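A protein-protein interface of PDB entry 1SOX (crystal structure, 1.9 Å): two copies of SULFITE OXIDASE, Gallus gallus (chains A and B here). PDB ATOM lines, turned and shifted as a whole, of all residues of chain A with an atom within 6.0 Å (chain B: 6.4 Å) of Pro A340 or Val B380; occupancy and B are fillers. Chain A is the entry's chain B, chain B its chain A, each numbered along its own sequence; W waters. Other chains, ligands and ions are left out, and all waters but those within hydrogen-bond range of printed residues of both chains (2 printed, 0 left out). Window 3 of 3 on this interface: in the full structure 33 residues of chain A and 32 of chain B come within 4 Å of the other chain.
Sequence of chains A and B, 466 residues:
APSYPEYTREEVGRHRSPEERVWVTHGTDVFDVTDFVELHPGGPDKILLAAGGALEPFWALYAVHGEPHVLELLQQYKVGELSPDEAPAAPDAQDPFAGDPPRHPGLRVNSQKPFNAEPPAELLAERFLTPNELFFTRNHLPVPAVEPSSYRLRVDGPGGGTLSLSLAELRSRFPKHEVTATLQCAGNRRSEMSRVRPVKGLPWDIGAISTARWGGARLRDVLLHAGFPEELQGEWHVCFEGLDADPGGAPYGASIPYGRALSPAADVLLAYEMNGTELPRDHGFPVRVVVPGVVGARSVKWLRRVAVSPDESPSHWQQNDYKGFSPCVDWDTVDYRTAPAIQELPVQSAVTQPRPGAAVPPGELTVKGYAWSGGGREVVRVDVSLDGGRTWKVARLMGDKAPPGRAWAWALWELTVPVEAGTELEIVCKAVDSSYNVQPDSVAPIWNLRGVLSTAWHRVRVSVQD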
ATOM      1  N   GLU A 312       8.551 -23.255  15.545  1.00  0.00           N
ATOM      2  CA  GLU A 312       8.736 -22.495  14.323  1.00  0.00           C
ATOM      3  C   GLU A 312       9.267 -21.106  14.680  1.00  0.00           C
ATOM      4  O   GLU A 312       9.056 -20.682  15.818  1.00  0.00           O
ATOM      5  CB  GLU A 312       7.369 -22.303  13.671  1.00  0.00           C
ATOM      6  CG  GLU A 312       7.084 -23.059  12.407  1.00  0.00           C
ATOM      7  CD  GLU A 312       5.882 -22.479  11.680  1.00  0.00           C
ATOM      8  OE1 GLU A 312       4.983 -21.955  12.386  1.00  0.00           O
ATOM      9  OE2 GLU A 312       5.891 -22.526  10.438  1.00  0.00           O
ATOM     10  N   TYR A 322       2.643 -15.096   4.539  1.00  0.00           N
ATOM     11  CA  TYR A 322       3.000 -16.247   3.708  1.00  0.00           C
ATOM     12  C   TYR A 322       2.267 -17.525   4.006  1.00  0.00           C
ATOM     13  O   TYR A 322       2.847 -18.577   4.337  1.00  0.00           O
ATOM     14  CB  TYR A 322       4.533 -16.452   3.817  1.00  0.00           C
ATOM     15  CG  TYR A 322       5.250 -15.202   3.321  1.00  0.00           C
ATOM     16  CD1 TYR A 322       5.009 -14.704   2.060  1.00  0.00           C
ATOM     17  CD2 TYR A 322       6.142 -14.510   4.143  1.00  0.00           C
ATOM     18  CE1 TYR A 322       5.626 -13.553   1.598  1.00  0.00           C
ATOM     19  CE2 TYR A 322       6.765 -13.365   3.672  1.00  0.00           C
ATOM     20  CZ  TYR A 322       6.524 -12.891   2.411  1.00  0.00           C
ATOM     21  OH  TYR A 322       7.120 -11.737   1.915  1.00  0.00           O
ATOM     22  N   LYS A 323       0.941 -17.502   3.948  1.00  0.00           N
ATOM     23  CA  LYS A 323       0.082 -18.663   4.155  1.00  0.00           C
ATOM     24  C   LYS A 323      -1.083 -18.579   3.148  1.00  0.00           C
ATOM     25  O   LYS A 323      -1.393 -17.470   2.705  1.00  0.00           O
ATOM     26  CB  LYS A 323      -0.490 -18.703   5.583  1.00  0.00           C
ATOM     27  CG  LYS A 323       0.613 -18.976   6.624  1.00  0.00           C
ATOM     28  CD  LYS A 323       0.041 -19.166   8.009  1.00  0.00           C
ATOM     29  CE  LYS A 323       1.137 -19.337   9.057  1.00  0.00           C
ATOM     30  NZ  LYS A 323       0.613 -20.017  10.275  1.00  0.00           N
ATOM     31  N   GLY A 324      -1.715 -19.700   2.855  1.00  0.00           N
ATOM     32  CA  GLY A 324      -2.828 -19.664   1.903  1.00  0.00           C
ATOM     33  C   GLY A 324      -4.130 -19.895   2.636  1.00  0.00           C
ATOM     34  O   GLY A 324      -4.186 -20.683   3.570  1.00  0.00           O
ATOM     35  N   TYR A 336      -4.342 -16.472  10.983  1.00  0.00           N
ATOM     36  CA  TYR A 336      -3.136 -17.167  10.563  1.00  0.00           C
ATOM     37  C   TYR A 336      -2.871 -18.458  11.293  1.00  0.00           C
ATOM     38  O   TYR A 336      -1.984 -19.229  10.893  1.00  0.00           O
ATOM     39  CB  TYR A 336      -1.909 -16.218  10.630  1.00  0.00           C
ATOM     40  CG  TYR A 336      -1.759 -15.471   9.324  1.00  0.00           C
ATOM     41  CD1 TYR A 336      -2.536 -14.355   9.062  1.00  0.00           C
ATOM     42  CD2 TYR A 336      -0.898 -15.904   8.323  1.00  0.00           C
ATOM     43  CE1 TYR A 336      -2.427 -13.666   7.864  1.00  0.00           C
ATOM     44  CE2 TYR A 336      -0.789 -15.227   7.129  1.00  0.00           C
ATOM     45  CZ  TYR A 336      -1.559 -14.100   6.901  1.00  0.00           C
ATOM     46  OH  TYR A 336      -1.456 -13.430   5.702  1.00  0.00           O
ATOM     47  N   ARG A 337      -3.601 -18.776  12.365  1.00  0.00           N
ATOM     48  CA  ARG A 337      -3.417 -20.038  13.069  1.00  0.00           C
ATOM     49  C   ARG A 337      -4.092 -21.202  12.336  1.00  0.00           C
ATOM     50  O   ARG A 337      -3.820 -22.367  12.648  1.00  0.00           O
ATOM     51  CB  ARG A 337      -4.017 -19.986  14.481  1.00  0.00           C
ATOM     52  CG  ARG A 337      -3.380 -18.910  15.364  1.00  0.00           C
ATOM     53  CD  ARG A 337      -4.450 -17.957  15.866  1.00  0.00           C
ATOM     54  NE  ARG A 337      -5.030 -18.251  17.122  1.00  0.00           N
ATOM     55  CZ  ARG A 337      -6.186 -17.965  17.686  1.00  0.00           C
ATOM     56  NH1 ARG A 337      -7.167 -17.326  17.071  1.00  0.00           N
ATOM     57  NH2 ARG A 337      -6.331 -18.397  18.937  1.00  0.00           N
ATOM     58  N   THR A 338      -4.941 -20.881  11.356  1.00  0.00           N
ATOM     59  CA  THR A 338      -5.715 -21.903  10.672  1.00  0.00           C
ATOM     60  C   THR A 338      -5.017 -22.489   9.450  1.00  0.00           C
ATOM     61  O   THR A 338      -5.584 -23.421   8.869  1.00  0.00           O
ATOM     62  CB  THR A 338      -7.090 -21.357  10.187  1.00  0.00           C
ATOM     63  OG1 THR A 338      -6.867 -20.408   9.148  1.00  0.00           O
ATOM     64  CG2 THR A 338      -7.840 -20.696  11.347  1.00  0.00           C
ATOM     65  N   ALA A 339      -3.880 -21.962   9.043  1.00  0.00           N
ATOM     66  CA  ALA A 339      -3.169 -22.529   7.880  1.00  0.00           C
ATOM     67  C   ALA A 339      -1.700 -22.704   8.235  1.00  0.00           C
ATOM     68  O   ALA A 339      -1.155 -22.055   9.145  1.00  0.00           O
ATOM     69  CB  ALA A 339      -3.329 -21.560   6.717  1.00  0.00           C
ATOM     70  N   PRO A 340      -1.003 -23.551   7.516  1.00  0.00           N
ATOM     71  CA  PRO A 340       0.429 -23.779   7.716  1.00  0.00           C
ATOM     72  C   PRO A 340       1.255 -22.780   6.937  1.00  0.00           C
ATOM     73  O   PRO A 340       0.888 -22.293   5.851  1.00  0.00           O
ATOM     74  CB  PRO A 340       0.678 -25.208   7.183  1.00  0.00           C
ATOM     75  CG  PRO A 340      -0.354 -25.288   6.084  1.00  0.00           C
ATOM     76  CD  PRO A 340      -1.550 -24.428   6.468  1.00  0.00           C
ATOM     77  N   ALA A 341       2.482 -22.500   7.412  1.00  0.00           N
ATOM     78  CA  ALA A 341       3.389 -21.621   6.686  1.00  0.00           C
ATOM     79  C   ALA A 341       3.680 -22.234   5.305  1.00  0.00           C
ATOM     80  O   ALA A 341       3.875 -23.451   5.249  1.00  0.00           O
ATOM     81  CB  ALA A 341       4.738 -21.519   7.387  1.00  0.00           C
ATOM     82  N   ILE A 342       3.778 -21.382   4.292  1.00  0.00           N
ATOM     83  CA  ILE A 342       4.154 -21.920   2.984  1.00  0.00           C
ATOM     84  C   ILE A 342       5.600 -22.424   3.066  1.00  0.00           C
ATOM     85  O   ILE A 342       6.472 -21.690   3.559  1.00  0.00           O
ATOM     86  CB  ILE A 342       4.052 -20.878   1.875  1.00  0.00           C
ATOM     87  CG1 ILE A 342       2.592 -20.430   1.688  1.00  0.00           C
ATOM     88  CG2 ILE A 342       4.610 -21.427   0.552  1.00  0.00           C
ATOM     89  CD1 ILE A 342       2.518 -19.155   0.836  1.00  0.00           C
ATOM     90  N   GLU B 378       0.141 -33.872   3.774  1.00  0.00           N
ATOM     91  CA  GLU B 378      -1.169 -33.875   4.433  1.00  0.00           C
ATOM     92  C   GLU B 378      -2.151 -32.943   3.724  1.00  0.00           C
ATOM     93  O   GLU B 378      -1.725 -32.070   2.979  1.00  0.00           O
ATOM     94  CB  GLU B 378      -1.025 -33.468   5.907  1.00  0.00           C
ATOM     95  CG  GLU B 378      -0.595 -32.022   6.083  1.00  0.00           C
ATOM     96  CD  GLU B 378      -0.788 -31.496   7.496  1.00  0.00           C
ATOM     97  OE1 GLU B 378      -1.334 -32.180   8.380  1.00  0.00           O
ATOM     98  OE2 GLU B 378      -0.369 -30.336   7.717  1.00  0.00           O
ATOM     99  N   VAL B 379      -3.424 -33.130   4.045  1.00  0.00           N
ATOM    100  CA  VAL B 379      -4.481 -32.246   3.556  1.00  0.00           C
ATOM    101  C   VAL B 379      -4.591 -31.063   4.534  1.00  0.00           C
ATOM    102  O   VAL B 379      -4.852 -31.357   5.709  1.00  0.00           O
ATOM    103  CB  VAL B 379      -5.851 -32.948   3.523  1.00  0.00           C
ATOM    104  CG1 VAL B 379      -6.985 -31.962   3.191  1.00  0.00           C
ATOM    105  CG2 VAL B 379      -5.872 -34.070   2.496  1.00  0.00           C
ATOM    106  N   VAL B 380      -4.329 -29.858   4.084  1.00  0.00           N
ATOM    107  CA  VAL B 380      -4.363 -28.721   5.000  1.00  0.00           C
ATOM    108  C   VAL B 380      -5.702 -28.003   5.005  1.00  0.00           C
ATOM    109  O   VAL B 380      -5.988 -27.266   5.952  1.00  0.00           O
ATOM    110  CB  VAL B 380      -3.231 -27.714   4.702  1.00  0.00           C
ATOM    111  CG1 VAL B 380      -1.903 -28.470   4.692  1.00  0.00           C
ATOM    112  CG2 VAL B 380      -3.421 -26.976   3.397  1.00  0.00           C
ATOM    113  N   ARG B 381      -6.522 -28.237   3.989  1.00  0.00           N
ATOM    114  CA  ARG B 381      -7.847 -27.588   3.961  1.00  0.00           C
ATOM    115  C   ARG B 381      -8.715 -28.261   2.882  1.00  0.00           C
ATOM    116  O   ARG B 381      -8.215 -28.696   1.847  1.00  0.00           O
ATOM    117  CB  ARG B 381      -7.725 -26.116   3.564  1.00  0.00           C
ATOM    118  CG  ARG B 381      -9.058 -25.350   3.851  1.00  0.00           C
ATOM    119  CD  ARG B 381      -8.894 -23.878   3.500  1.00  0.00           C
ATOM    120  NE  ARG B 381      -8.946 -23.622   2.069  1.00  0.00           N
ATOM    121  CZ  ARG B 381      -7.957 -23.223   1.296  1.00  0.00           C
ATOM    122  NH1 ARG B 381      -6.732 -22.981   1.768  1.00  0.00           N
ATOM    123  NH2 ARG B 381      -8.184 -23.022   0.013  1.00  0.00           N
ATOM    124  N   VAL B 382     -10.008 -28.285   3.112  1.00  0.00           N
ATOM    125  CA  VAL B 382     -10.985 -28.736   2.117  1.00  0.00           C
ATOM    126  C   VAL B 382     -12.058 -27.637   2.032  1.00  0.00           C
ATOM    127  O   VAL B 382     -12.600 -27.262   3.075  1.00  0.00           O
ATOM    128  CB  VAL B 382     -11.670 -30.034   2.545  1.00  0.00           C
ATOM    129  CG1 VAL B 382     -12.822 -30.361   1.592  1.00  0.00           C
ATOM    130  CG2 VAL B 382     -10.701 -31.219   2.612  1.00  0.00           C
ATOM    131  N   LEU B 397     -11.877 -30.928   9.331  1.00  0.00           N
ATOM    132  CA  LEU B 397     -11.060 -32.094   9.021  1.00  0.00           C
ATOM    133  C   LEU B 397     -11.066 -33.000  10.241  1.00  0.00           C
ATOM    134  O   LEU B 397     -10.861 -32.504  11.349  1.00  0.00           O
ATOM    135  CB  LEU B 397      -9.653 -31.699   8.601  1.00  0.00           C
ATOM    136  CG  LEU B 397      -9.492 -30.804   7.394  1.00  0.00           C
ATOM    137  CD1 LEU B 397      -8.026 -30.539   7.069  1.00  0.00           C
ATOM    138  CD2 LEU B 397     -10.203 -31.397   6.169  1.00  0.00           C
ATOM    139  N   VAL B 432      -6.599 -28.940  -0.562  1.00  0.00           N
ATOM    140  CA  VAL B 432      -5.278 -28.310  -0.671  1.00  0.00           C
ATOM    141  C   VAL B 432      -4.283 -29.087   0.184  1.00  0.00           C
ATOM    142  O   VAL B 432      -4.593 -29.396   1.366  1.00  0.00           O
ATOM    143  CB  VAL B 432      -5.303 -26.850  -0.155  1.00  0.00           C
ATOM    144  CG1 VAL B 432      -3.938 -26.191  -0.374  1.00  0.00           C
ATOM    145  CG2 VAL B 432      -6.341 -26.026  -0.909  1.00  0.00           C
ATOM    146  N   ASP B 433      -3.098 -29.424  -0.361  1.00  0.00           N
ATOM    147  CA  ASP B 433      -2.193 -30.240   0.456  1.00  0.00           C
ATOM    148  C   ASP B 433      -1.105 -29.380   1.086  1.00  0.00           C
ATOM    149  O   ASP B 433      -1.033 -28.161   0.947  1.00  0.00           O
ATOM    150  CB  ASP B 433      -1.675 -31.471  -0.320  1.00  0.00           C
ATOM    151  CG  ASP B 433      -0.638 -31.188  -1.374  1.00  0.00           C
ATOM    152  OD1 ASP B 433      -0.067 -30.098  -1.459  1.00  0.00           O
ATOM    153  OD2 ASP B 433      -0.277 -32.120  -2.165  1.00  0.00           O
ATOM    154  N   SER B 434      -0.157 -30.029   1.787  1.00  0.00           N
ATOM    155  CA  SER B 434       0.889 -29.304   2.492  1.00  0.00           C
ATOM    156  C   SER B 434       1.927 -28.597   1.653  1.00  0.00           C
ATOM    157  O   SER B 434       2.625 -27.719   2.181  1.00  0.00           O
ATOM    158  CB  SER B 434       1.513 -30.286   3.492  1.00  0.00           C
ATOM    159  OG  SER B 434       2.230 -31.286   2.756  1.00  0.00           O
ATOM    160  N   SER B 435       1.978 -28.864   0.350  1.00  0.00           N
ATOM    161  CA  SER B 435       2.778 -28.176  -0.639  1.00  0.00           C
ATOM    162  C   SER B 435       1.941 -27.153  -1.408  1.00  0.00           C
ATOM    163  O   SER B 435       2.369 -26.489  -2.361  1.00  0.00           O
ATOM    164  CB  SER B 435       3.404 -29.175  -1.624  1.00  0.00           C
ATOM    165  OG  SER B 435       4.048 -28.508  -2.699  1.00  0.00           O
ATOM    166  N   TYR B 436       0.738 -26.953  -0.879  1.00  0.00           N
ATOM    167  CA  TYR B 436      -0.269 -26.051  -1.433  1.00  0.00           C
ATOM    168  C   TYR B 436      -0.632 -26.407  -2.879  1.00  0.00           C
ATOM    169  O   TYR B 436      -1.051 -25.562  -3.680  1.00  0.00           O
ATOM    170  CB  TYR B 436       0.111 -24.578  -1.291  1.00  0.00           C
ATOM    171  CG  TYR B 436      -0.155 -24.044   0.114  1.00  0.00           C
ATOM    172  CD1 TYR B 436      -1.410 -23.532   0.427  1.00  0.00           C
ATOM    173  CD2 TYR B 436       0.820 -24.010   1.095  1.00  0.00           C
ATOM    174  CE1 TYR B 436      -1.679 -23.022   1.678  1.00  0.00           C
ATOM    175  CE2 TYR B 436       0.561 -23.501   2.374  1.00  0.00           C
ATOM    176  CZ  TYR B 436      -0.692 -23.013   2.653  1.00  0.00           C
ATOM    177  OH  TYR B 436      -0.995 -22.492   3.907  1.00  0.00           O
HETATM  178  O   HOH W   1      -5.752 -22.512   4.513  1.00  0.00           O
HETATM  179  O   HOH W   2      -5.367 -24.606   6.402  1.00  0.00           O
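No position is printed for both chains.
The backbone carbonyl oxygen (O) of Pro A340 lies within hydrogen-bond range of the side-chain hydroxyl (OH) of Tyr B436 (2.7 Å).
The backbone NH (N) of Gly A324 sits at hydrogen-bond distance from the side-chain hydroxyl (OH) of Tyr B436 (3.1 Å).
Val B380 touches just one residue of chain A: Pro A340 (3.8 Å).
Of the printed residues of chain B, Ala A339 touches Tyr B436.
Of the printed residues of chain B, Ile A342 touches Tyr B436.
Val B382 touches none of the printed residues of chain A.
Among the printed residues, pairs that only touch across the chains: Ile A342 with Tyr B436 (3.7 Å), Ala A339 with Tyr B436 (3.8 Å), Pro A340 with Val B380 (3.8 Å), Gly A324 with Arg B381 (3.9 Å) and Lys A323 with Tyr B436 (3.99 Å).
Water W1 lies within hydrogen-bond range of O of Gly A324 (2.6 Å) and NH1 of Arg B381 (3.0 Å).
Water W2 lies within hydrogen-bond range of O of Thr A338 and O of Val B380.
Of the 11 printed residues of chain B, 3 touch a printed residue of chain A.
Printed residues of chain A that touch a printed residue of chain B: Lys A323, Gly A324, Ala A339, Pro A340 and Ile A342.
Hydrophobic or aromatic side chains of chain A within 4 Å of the printed part of chain B: Ala A339, Pro A340 and Ile A342.
Among the printed residues, no Asp or Glu carboxylate lies within 4 Å of a Lys or Arg side-chain nitrogen of the other chain.
The backbone carbonyl oxygen of Arg B381 lies within hydrogen-bond range of the backbone NH of Val B432 (2.9 Å).
The side-chain amino group (NZ) of Lys A323 is in hydrogen-bond range of the backbone carbonyl oxygen (O) of Ala A339 (2.9 Å).
NZ of Lys A323 is in hydrogen-bond range of O of Tyr A336 (2.8 Å).
N of Tyr B436 is in hydrogen-bond range of OD1 of Asp B433.
The backbone NH of Val B380 lies within hydrogen-bond range of the backbone carbonyl oxygen of Val B432 (2.8 Å).
O of Tyr A322 is in hydrogen-bond range of N of Ile A342.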
